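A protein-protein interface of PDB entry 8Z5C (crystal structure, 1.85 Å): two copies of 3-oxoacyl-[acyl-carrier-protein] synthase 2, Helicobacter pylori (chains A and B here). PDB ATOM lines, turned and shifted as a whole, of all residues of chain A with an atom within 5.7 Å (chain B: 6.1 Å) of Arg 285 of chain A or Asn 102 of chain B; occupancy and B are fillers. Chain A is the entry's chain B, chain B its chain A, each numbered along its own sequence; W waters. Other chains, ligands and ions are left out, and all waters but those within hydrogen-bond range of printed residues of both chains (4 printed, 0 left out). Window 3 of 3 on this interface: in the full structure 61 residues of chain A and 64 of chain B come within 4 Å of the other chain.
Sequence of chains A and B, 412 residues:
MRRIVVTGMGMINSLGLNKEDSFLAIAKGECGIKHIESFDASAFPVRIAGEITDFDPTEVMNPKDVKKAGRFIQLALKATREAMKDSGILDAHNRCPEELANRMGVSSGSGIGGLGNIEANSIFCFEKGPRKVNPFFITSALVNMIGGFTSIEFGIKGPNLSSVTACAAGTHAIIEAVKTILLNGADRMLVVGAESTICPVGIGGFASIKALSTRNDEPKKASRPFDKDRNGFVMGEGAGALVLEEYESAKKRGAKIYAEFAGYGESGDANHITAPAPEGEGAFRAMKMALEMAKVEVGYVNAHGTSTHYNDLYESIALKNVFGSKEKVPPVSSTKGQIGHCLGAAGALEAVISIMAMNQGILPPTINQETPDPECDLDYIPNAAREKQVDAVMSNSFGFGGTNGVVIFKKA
Among the printed residues, pairs that only touch across the chains: Ser 267 of chain A with Lys 157 of chain B (3.8 Å), Ser 267 of chain A with Gly 158 of chain B (3.5 Å), Asp 269 of chain A with Lys 157 of chain B (3.5 Å) and Arg 285 of chain A with Asn 102 of chain B (3.6 Å).
Water W3 bridges the backbone carbonyl oxygen of Gly 185 of chain B and the side-chain sulfur of Met 289 of chain A. Water W2 bridges the side-chain carboxylate (OE2) of Glu 281 of chain A and the side-chain amide oxygen (OD1) of Asn 102 of chain B. Water W4 lies within hydrogen-bond range of NH1 of Arg 103 of chain B (2.9 Å) and SD of Met 289 of chain A (3.4 Å). Water W1 bridges NH1 of Arg 285 of chain A (3.0 Å) and O of Asn 102 of chain B (3.1 Å).
The backbone carbonyl oxygen (O) of Gly 158 of chain B sits at hydrogen-bond distance from the backbone NH (N) of Gly 268 of chain A (3.1 Å). The backbone carbonyl oxygen (O) of Lys 157 of chain B lies within hydrogen-bond range of the guanidinium group (NH1) of Arg 285 of chain A (2.9 Å). O of Lys 157 of chain B lies within hydrogen-bond range of N of Gly 268 of chain A (3.0 Å).
O of Ala 101 of chain B sits at hydrogen-bond distance from N of Lys 157 of chain B (2.9 Å). O of Gly 282 of chain A lies within hydrogen-bond range of OG of Ser 267 of chain A, at 2.7 Å. The backbone carbonyl oxygen of Gly 268 of chain A is in hydrogen-bond range of the guanidinium group of Arg 285 of chain A, 3.0 Å away. The side-chain carboxylate of Glu 281 of chain A lies within salt-bridge range of the guanidinium group of Arg 285 of chain A (2.6 Å). The backbone NH of Lys 157 of chain B lies within hydrogen-bond range of the backbone carbonyl oxygen of Met 104 of chain B (3.2 Å). The backbone carbonyl oxygen (O) of Ala 101 of chain B is in hydrogen-bond range of the backbone NH (N) of Gly 158 of chain B (3.5 Å).
Of chain A, only Arg 285 (3.6 Å) comes within 4 Å of Asn 102 of chain B. Of the printed residues of chain B, Ser 267 of chain A touches Lys 157 and Gly 158. Of the printed residues of chain B, Asp 269 of chain A touches Lys 157. Of the printed residues of chain B, Gly 268 of chain A touches Lys 157 (3.0 Å) and Gly 158 (3.1 Å). Printed residues of chain A within 4 Å of Lys 157 of chain B: Ser 267, Gly 268, Asp 269 and Arg 285. Of the printed residues of chain A, Gly 158 of chain B touches Ser 267 and Gly 268. Gly 185 of chain B touches none of the printed residues of chain A. The nearest residue of chain A that does not touch Asn 102 of chain B is Glu 281 of chain A (4.8 Å). The nearest printed residue of chain B that does not touch Asp 269 of chain A is Ile 156 of chain B (5.7 Å).
No position is printed for both chains.
Of the 15 printed residues of chain A, 4 touch a printed residue of chain B. Along chain A the printed residues that touch a printed residue of chain B span positions 267 to 285.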
ATOM      1  N   GLY A 265     -21.069  10.789  11.003  1.00  0.00           N
ATOM      2  CA  GLY A 265     -20.879  11.186   9.622  1.00  0.00           C
ATOM      3  C   GLY A 265     -19.905  10.237   8.961  1.00  0.00           C
ATOM      4  O   GLY A 265     -18.982   9.722   9.596  1.00  0.00           O
ATOM      5  N   SER A 267     -17.826   9.595   5.029  1.00  0.00           N
ATOM      6  CA  SER A 267     -17.533  10.192   3.732  1.00  0.00           C
ATOM      7  C   SER A 267     -16.353   9.476   3.091  1.00  0.00           C
ATOM      8  O   SER A 267     -15.661   8.689   3.733  1.00  0.00           O
ATOM      9  CB  SER A 267     -17.255  11.684   3.883  1.00  0.00           C
ATOM     10  OG  SER A 267     -16.017  11.868   4.533  1.00  0.00           O
ATOM     11  N   GLY A 268     -16.141   9.755   1.806  1.00  0.00           N
ATOM     12  CA  GLY A 268     -14.937   9.309   1.114  1.00  0.00           C
ATOM     13  C   GLY A 268     -14.226  10.475   0.459  1.00  0.00           C
ATOM     14  O   GLY A 268     -14.859  11.342  -0.142  1.00  0.00           O
ATOM     15  N   ASP A 269     -12.894  10.494   0.597  1.00  0.00           N
ATOM     16  CA  ASP A 269     -12.078  11.532  -0.043  1.00  0.00           C
ATOM     17  C   ASP A 269     -12.183  11.466  -1.561  1.00  0.00           C
ATOM     18  O   ASP A 269     -12.226  12.501  -2.239  1.00  0.00           O
ATOM     19  CB  ASP A 269     -10.611  11.351   0.348  1.00  0.00           C
ATOM     20  CG  ASP A 269     -10.316  11.750   1.782  1.00  0.00           C
ATOM     21  OD1 ASP A 269     -11.240  12.149   2.523  1.00  0.00           O
ATOM     22  OD2 ASP A 269      -9.142  11.603   2.174  1.00  0.00           O
ATOM     23  N   GLY A 280      -8.023  18.294   4.339  1.00  0.00           N
ATOM     24  CA  GLY A 280      -8.872  17.342   5.040  1.00  0.00           C
ATOM     25  C   GLY A 280     -10.301  17.424   4.556  1.00  0.00           C
ATOM     26  O   GLY A 280     -11.239  17.330   5.358  1.00  0.00           O
ATOM     27  N   GLU A 281     -10.485  17.595   3.245  1.00  0.00           N
ATOM     28  CA  GLU A 281     -11.796  17.940   2.704  1.00  0.00           C
ATOM     29  C   GLU A 281     -12.843  16.877   3.047  1.00  0.00           C
ATOM     30  O   GLU A 281     -13.973  17.204   3.423  1.00  0.00           O
ATOM     31  CB  GLU A 281     -11.668  18.146   1.184  1.00  0.00           C
ATOM     32  CG  GLU A 281     -12.951  18.587   0.502  1.00  0.00           C
ATOM     33  CD  GLU A 281     -13.902  17.472   0.159  1.00  0.00           C
ATOM     34  OE1 GLU A 281     -13.489  16.295   0.032  1.00  0.00           O
ATOM     35  OE2 GLU A 281     -15.096  17.783   0.103  1.00  0.00           O
ATOM     36  N   GLY A 282     -12.489  15.594   2.941  1.00  0.00           N
ATOM     37  CA  GLY A 282     -13.463  14.554   3.266  1.00  0.00           C
ATOM     38  C   GLY A 282     -13.690  14.418   4.763  1.00  0.00           C
ATOM     39  O   GLY A 282     -14.811  14.131   5.217  1.00  0.00           O
ATOM     40  N   ALA A 283     -12.628  14.606   5.546  1.00  0.00           N
ATOM     41  CA  ALA A 283     -12.749  14.625   6.999  1.00  0.00           C
ATOM     42  C   ALA A 283     -13.679  15.739   7.444  1.00  0.00           C
ATOM     43  O   ALA A 283     -14.502  15.554   8.344  1.00  0.00           O
ATOM     44  CB  ALA A 283     -11.362  14.809   7.617  1.00  0.00           C
ATOM     45  N   PHE A 284     -13.539  16.913   6.823  1.00  0.00           N
ATOM     46  CA  PHE A 284     -14.414  18.053   7.081  1.00  0.00           C
ATOM     47  C   PHE A 284     -15.879  17.673   6.906  1.00  0.00           C
ATOM     48  O   PHE A 284     -16.726  17.954   7.765  1.00  0.00           O
ATOM     49  CB  PHE A 284     -14.036  19.180   6.108  1.00  0.00           C
ATOM     50  CG  PHE A 284     -14.997  20.335   6.096  1.00  0.00           C
ATOM     51  CD1 PHE A 284     -14.937  21.319   7.077  1.00  0.00           C
ATOM     52  CD2 PHE A 284     -15.989  20.417   5.123  1.00  0.00           C
ATOM     53  CE1 PHE A 284     -15.827  22.384   7.061  1.00  0.00           C
ATOM     54  CE2 PHE A 284     -16.892  21.463   5.110  1.00  0.00           C
ATOM     55  CZ  PHE A 284     -16.811  22.451   6.078  1.00  0.00           C
ATOM     56  N   ARG A 285     -16.190  17.030   5.779  1.00  0.00           N
ATOM     57  CA  ARG A 285     -17.574  16.696   5.473  1.00  0.00           C
ATOM     58  C   ARG A 285     -18.125  15.702   6.486  1.00  0.00           C
ATOM     59  O   ARG A 285     -19.277  15.826   6.923  1.00  0.00           O
ATOM     60  CB  ARG A 285     -17.654  16.145   4.049  1.00  0.00           C
ATOM     61  CG  ARG A 285     -17.738  17.240   2.966  1.00  0.00           C
ATOM     62  CD  ARG A 285     -17.989  16.612   1.583  1.00  0.00           C
ATOM     63  NE  ARG A 285     -16.784  15.981   1.063  1.00  0.00           N
ATOM     64  CZ  ARG A 285     -16.692  14.676   0.818  1.00  0.00           C
ATOM     65  NH1 ARG A 285     -17.724  13.864   1.006  1.00  0.00           N
ATOM     66  NH2 ARG A 285     -15.537  14.175   0.395  1.00  0.00           N
ATOM     67  N   ALA A 286     -17.313  14.714   6.877  1.00  0.00           N
ATOM     68  CA  ALA A 286     -17.766  13.713   7.848  1.00  0.00           C
ATOM     69  C   ALA A 286     -18.046  14.355   9.203  1.00  0.00           C
ATOM     70  O   ALA A 286     -19.043  14.045   9.864  1.00  0.00           O
ATOM     71  CB  ALA A 286     -16.715  12.606   7.994  1.00  0.00           C
ATOM     72  N   MET A 287     -17.144  15.229   9.610  1.00  0.00           N
ATOM     73  CA  MET A 287     -17.307  15.945  10.897  1.00  0.00           C
ATOM     74  C   MET A 287     -18.545  16.855  10.855  1.00  0.00           C
ATOM     75  O   MET A 287     -19.330  16.829  11.778  1.00  0.00           O
ATOM     76  CB  MET A 287     -16.040  16.754  11.184  1.00  0.00           C
ATOM     77  CG  MET A 287     -14.873  15.924  11.637  1.00  0.00           C
ATOM     78  SD  MET A 287     -13.600  16.977  12.364  1.00  0.00           S
ATOM     79  CE  MET A 287     -12.646  17.345  10.896  1.00  0.00           C
ATOM     80  N   LYS A 288     -18.686  17.617   9.772  1.00  0.00           N
ATOM     81  CA  LYS A 288     -19.881  18.446   9.614  1.00  0.00           C
ATOM     82  C   LYS A 288     -21.163  17.647   9.736  1.00  0.00           C
ATOM     83  O   LYS A 288     -22.098  18.089  10.410  1.00  0.00           O
ATOM     84  CB  LYS A 288     -19.880  19.192   8.277  1.00  0.00           C
ATOM     85  CG  LYS A 288     -19.047  20.422   8.242  1.00  0.00           C
ATOM     86  CD  LYS A 288     -19.691  21.431   9.201  1.00  0.00           C
ATOM     87  CE  LYS A 288     -19.815  22.833   8.618  1.00  0.00           C
ATOM     88  NZ  LYS A 288     -19.200  23.832   9.560  1.00  0.00           N
ATOM     89  N   MET A 289     -21.257  16.492   9.057  1.00  0.00           N
ATOM     90  CA  MET A 289     -22.531  15.785   9.135  1.00  0.00           C
ATOM     91  C   MET A 289     -22.781  15.205  10.515  1.00  0.00           C
ATOM     92  O   MET A 289     -23.940  15.114  10.939  1.00  0.00           O
ATOM     93  CB  MET A 289     -22.681  14.690   8.074  1.00  0.00           C
ATOM     94  CG  MET A 289     -22.722  15.230   6.652  1.00  0.00           C
ATOM     95  SD  MET A 289     -22.582  13.888   5.480  1.00  0.00           S
ATOM     96  CE  MET A 289     -20.822  13.536   5.481  1.00  0.00           C
ATOM     97  N   ALA A 290     -21.730  14.801  11.227  1.00  0.00           N
ATOM     98  CA  ALA A 290     -21.940  14.319  12.586  1.00  0.00           C
ATOM     99  C   ALA A 290     -22.427  15.449  13.492  1.00  0.00           C
ATOM    100  O   ALA A 290     -23.392  15.281  14.249  1.00  0.00           O
ATOM    101  CB  ALA A 290     -20.649  13.704  13.132  1.00  0.00           C
ATOM    102  N   PRO B  97     -21.253  13.448 -11.751  1.00  0.00           N
ATOM    103  CA  PRO B  97     -21.237  14.916 -11.790  1.00  0.00           C
ATOM    104  C   PRO B  97     -20.829  15.477 -10.435  1.00  0.00           C
ATOM    105  O   PRO B  97     -21.209  14.943  -9.389  1.00  0.00           O
ATOM    106  CB  PRO B  97     -22.683  15.281 -12.145  1.00  0.00           C
ATOM    107  CG  PRO B  97     -23.178  14.120 -12.906  1.00  0.00           C
ATOM    108  CD  PRO B  97     -22.515  12.899 -12.273  1.00  0.00           C
ATOM    109  N   GLU B  98     -20.032  16.552 -10.459  1.00  0.00           N
ATOM    110  CA  GLU B  98     -19.423  17.056  -9.225  1.00  0.00           C
ATOM    111  C   GLU B  98     -20.463  17.513  -8.212  1.00  0.00           C
ATOM    112  O   GLU B  98     -20.270  17.340  -7.003  1.00  0.00           O
ATOM    113  CB  GLU B  98     -18.450  18.199  -9.524  1.00  0.00           C
ATOM    114  CG  GLU B  98     -17.495  17.916 -10.669  1.00  0.00           C
ATOM    115  CD  GLU B  98     -16.995  19.185 -11.343  1.00  0.00           C
ATOM    116  OE1 GLU B  98     -16.918  20.231 -10.661  1.00  0.00           O
ATOM    117  OE2 GLU B  98     -16.676  19.132 -12.553  1.00  0.00           O
ATOM    118  N   GLU B  99     -21.565  18.118  -8.675  1.00  0.00           N
ATOM    119  CA  GLU B  99     -22.553  18.600  -7.720  1.00  0.00           C
ATOM    120  C   GLU B  99     -23.319  17.461  -7.055  1.00  0.00           C
ATOM    121  O   GLU B  99     -24.055  17.715  -6.094  1.00  0.00           O
ATOM    122  CB  GLU B  99     -23.565  19.535  -8.395  1.00  0.00           C
ATOM    123  CG  GLU B  99     -24.388  18.854  -9.474  1.00  0.00           C
ATOM    124  CD  GLU B  99     -23.693  18.761 -10.822  1.00  0.00           C
ATOM    125  OE1 GLU B  99     -22.448  18.943 -10.904  1.00  0.00           O
ATOM    126  OE2 GLU B  99     -24.405  18.450 -11.796  1.00  0.00           O
ATOM    127  N   LEU B 100     -23.189  16.227  -7.560  1.00  0.00           N
ATOM    128  CA  LEU B 100     -23.857  15.057  -7.004  1.00  0.00           C
ATOM    129  C   LEU B 100     -22.914  14.117  -6.260  1.00  0.00           C
ATOM    130  O   LEU B 100     -23.383  13.138  -5.661  1.00  0.00           O
ATOM    131  CB  LEU B 100     -24.557  14.270  -8.124  1.00  0.00           C
ATOM    132  CG  LEU B 100     -25.500  15.103  -8.978  1.00  0.00           C
ATOM    133  CD1 LEU B 100     -26.112  14.230 -10.065  1.00  0.00           C
ATOM    134  CD2 LEU B 100     -26.572  15.712  -8.100  1.00  0.00           C
ATOM    135  N   ALA B 101     -21.615  14.401  -6.277  1.00  0.00           N
ATOM    136  CA  ALA B 101     -20.611  13.448  -5.808  1.00  0.00           C
ATOM    137  C   ALA B 101     -20.714  13.215  -4.312  1.00  0.00           C
ATOM    138  O   ALA B 101     -20.473  12.095  -3.835  1.00  0.00           O
ATOM    139  CB  ALA B 101     -19.215  13.958  -6.164  1.00  0.00           C
ATOM    140  N   ASN B 102     -21.057  14.257  -3.550  1.00  0.00           N
ATOM    141  CA  ASN B 102     -21.111  14.112  -2.104  1.00  0.00           C
ATOM    142  C   ASN B 102     -22.265  13.225  -1.657  1.00  0.00           C
ATOM    143  O   ASN B 102     -22.242  12.764  -0.517  1.00  0.00           O
ATOM    144  CB  ASN B 102     -21.216  15.480  -1.416  1.00  0.00           C
ATOM    145  CG  ASN B 102     -19.952  16.322  -1.564  1.00  0.00           C
ATOM    146  OD1 ASN B 102     -18.905  15.822  -1.960  1.00  0.00           O
ATOM    147  ND2 ASN B 102     -20.046  17.605  -1.213  1.00  0.00           N
ATOM    148  N   ARG B 103     -23.251  12.956  -2.518  1.00  0.00           N
ATOM    149  CA  ARG B 103     -24.419  12.175  -2.123  1.00  0.00           C
ATOM    150  C   ARG B 103     -24.428  10.774  -2.720  1.00  0.00           C
ATOM    151  O   ARG B 103     -25.424  10.051  -2.585  1.00  0.00           O
ATOM    152  CB  ARG B 103     -25.718  12.919  -2.462  1.00  0.00           C
ATOM    153  CG  ARG B 103     -25.895  14.164  -1.584  1.00  0.00           C
ATOM    154  CD  ARG B 103     -26.212  13.753  -0.142  1.00  0.00           C
ATOM    155  NE  ARG B 103     -27.487  13.046  -0.046  1.00  0.00           N
ATOM    156  CZ  ARG B 103     -28.014  12.609   1.092  1.00  0.00           C
ATOM    157  NH1 ARG B 103     -27.358  12.692   2.238  1.00  0.00           N
ATOM    158  NH2 ARG B 103     -29.218  12.058   1.074  1.00  0.00           N
ATOM    159  N   MET B 104     -23.335  10.347  -3.330  1.00  0.00           N
ATOM    160  CA  MET B 104     -23.221   8.974  -3.808  1.00  0.00           C
ATOM    161  C   MET B 104     -21.990   8.329  -3.209  1.00  0.00           C
ATOM    162  O   MET B 104     -20.877   8.842  -3.354  1.00  0.00           O
ATOM    163  CB  MET B 104     -23.255   8.908  -5.339  1.00  0.00           C
ATOM    164  CG  MET B 104     -23.228   7.479  -5.896  1.00  0.00           C
ATOM    165  SD  MET B 104     -23.119   7.429  -7.696  1.00  0.00           S
ATOM    166  CE  MET B 104     -23.883   5.836  -7.998  1.00  0.00           C
ATOM    167  N   GLY B 105     -22.205   7.226  -2.496  1.00  0.00           N
ATOM    168  CA  GLY B 105     -21.137   6.511  -1.842  1.00  0.00           C
ATOM    169  C   GLY B 105     -20.885   5.170  -2.498  1.00  0.00           C
ATOM    170  O   GLY B 105     -21.357   4.892  -3.599  1.00  0.00           O
ATOM    171  N   GLY B 155     -15.179   9.381  -8.834  1.00  0.00           N
ATOM    172  CA  GLY B 155     -15.355  10.654  -8.141  1.00  0.00           C
ATOM    173  C   GLY B 155     -16.590  10.672  -7.268  1.00  0.00           C
ATOM    174  O   GLY B 155     -17.324  11.671  -7.246  1.00  0.00           O
ATOM    175  N   ILE B 156     -16.851   9.579  -6.552  1.00  0.00           N
ATOM    176  CA  ILE B 156     -18.005   9.485  -5.657  1.00  0.00           C
ATOM    177  C   ILE B 156     -17.517   9.556  -4.211  1.00  0.00           C
ATOM    178  O   ILE B 156     -16.642   8.789  -3.787  1.00  0.00           O
ATOM    179  CB  ILE B 156     -18.852   8.223  -5.936  1.00  0.00           C
ATOM    180  CG1 ILE B 156     -18.034   6.935  -5.860  1.00  0.00           C
ATOM    181  CG2 ILE B 156     -19.545   8.312  -7.302  1.00  0.00           C
ATOM    182  CD1 ILE B 156     -18.857   5.714  -6.350  1.00  0.00           C
ATOM    183  N   LYS B 157     -18.080  10.491  -3.464  1.00  0.00           N
ATOM    184  CA  LYS B 157     -17.521  10.950  -2.201  1.00  0.00           C
ATOM    185  C   LYS B 157     -18.429  10.689  -1.014  1.00  0.00           C
ATOM    186  O   LYS B 157     -18.127  11.156   0.084  1.00  0.00           O
ATOM    187  CB  LYS B 157     -17.225  12.455  -2.281  1.00  0.00           C
ATOM    188  CG  LYS B 157     -16.420  12.834  -3.516  1.00  0.00           C
ATOM    189  CD  LYS B 157     -15.985  14.294  -3.453  1.00  0.00           C
ATOM    190  CE  LYS B 157     -14.552  14.499  -3.873  1.00  0.00           C
ATOM    191  NZ  LYS B 157     -14.492  15.543  -4.948  1.00  0.00           N
ATOM    192  N   GLY B 158     -19.540   9.990  -1.203  1.00  0.00           N
ATOM    193  CA  GLY B 158     -20.409   9.686  -0.095  1.00  0.00           C
ATOM    194  C   GLY B 158     -19.830   8.604   0.793  1.00  0.00           C
ATOM    195  O   GLY B 158     -18.647   8.261   0.690  1.00  0.00           O
ATOM    196  N   PRO B 159     -20.662   8.049   1.686  1.00  0.00           N
ATOM    197  CA  PRO B 159     -20.171   7.038   2.627  1.00  0.00           C
ATOM    198  C   PRO B 159     -19.484   5.907   1.886  1.00  0.00           C
ATOM    199  O   PRO B 159     -19.965   5.425   0.861  1.00  0.00           O
ATOM    200  CB  PRO B 159     -21.441   6.560   3.339  1.00  0.00           C
ATOM    201  CG  PRO B 159     -22.380   7.744   3.253  1.00  0.00           C
ATOM    202  CD  PRO B 159     -22.064   8.414   1.928  1.00  0.00           C
ATOM    203  N   GLY B 185     -28.332   9.017   4.441  1.00  0.00           N
ATOM    204  CA  GLY B 185     -26.901   9.246   4.356  1.00  0.00           C
ATOM    205  C   GLY B 185     -26.378   9.336   2.938  1.00  0.00           C
ATOM    206  O   GLY B 185     -25.238   9.756   2.725  1.00  0.00           O
ATOM    207  N   ALA B 186     -27.196   8.951   1.963  1.00  0.00           N
ATOM    208  CA  ALA B 186     -26.831   9.057   0.559  1.00  0.00           C
ATOM    209  C   ALA B 186     -28.098   8.953  -0.275  1.00  0.00           C
ATOM    210  O   ALA B 186     -29.124   8.436   0.184  1.00  0.00           O
ATOM    211  CB  ALA B 186     -25.824   7.965   0.149  1.00  0.00           C
HETATM  212  O   HOH W   1     -20.569  13.931   1.794  1.00  0.00           O
HETATM  213  O   HOH W   2     -16.569  17.345  -2.193  1.00  0.00           O
HETATM  214  O   HOH W   3     -23.392  11.228   4.127  1.00  0.00           O
HETATM  215  O   HOH W   4     -24.820  13.970   2.947  1.00  0.00           O
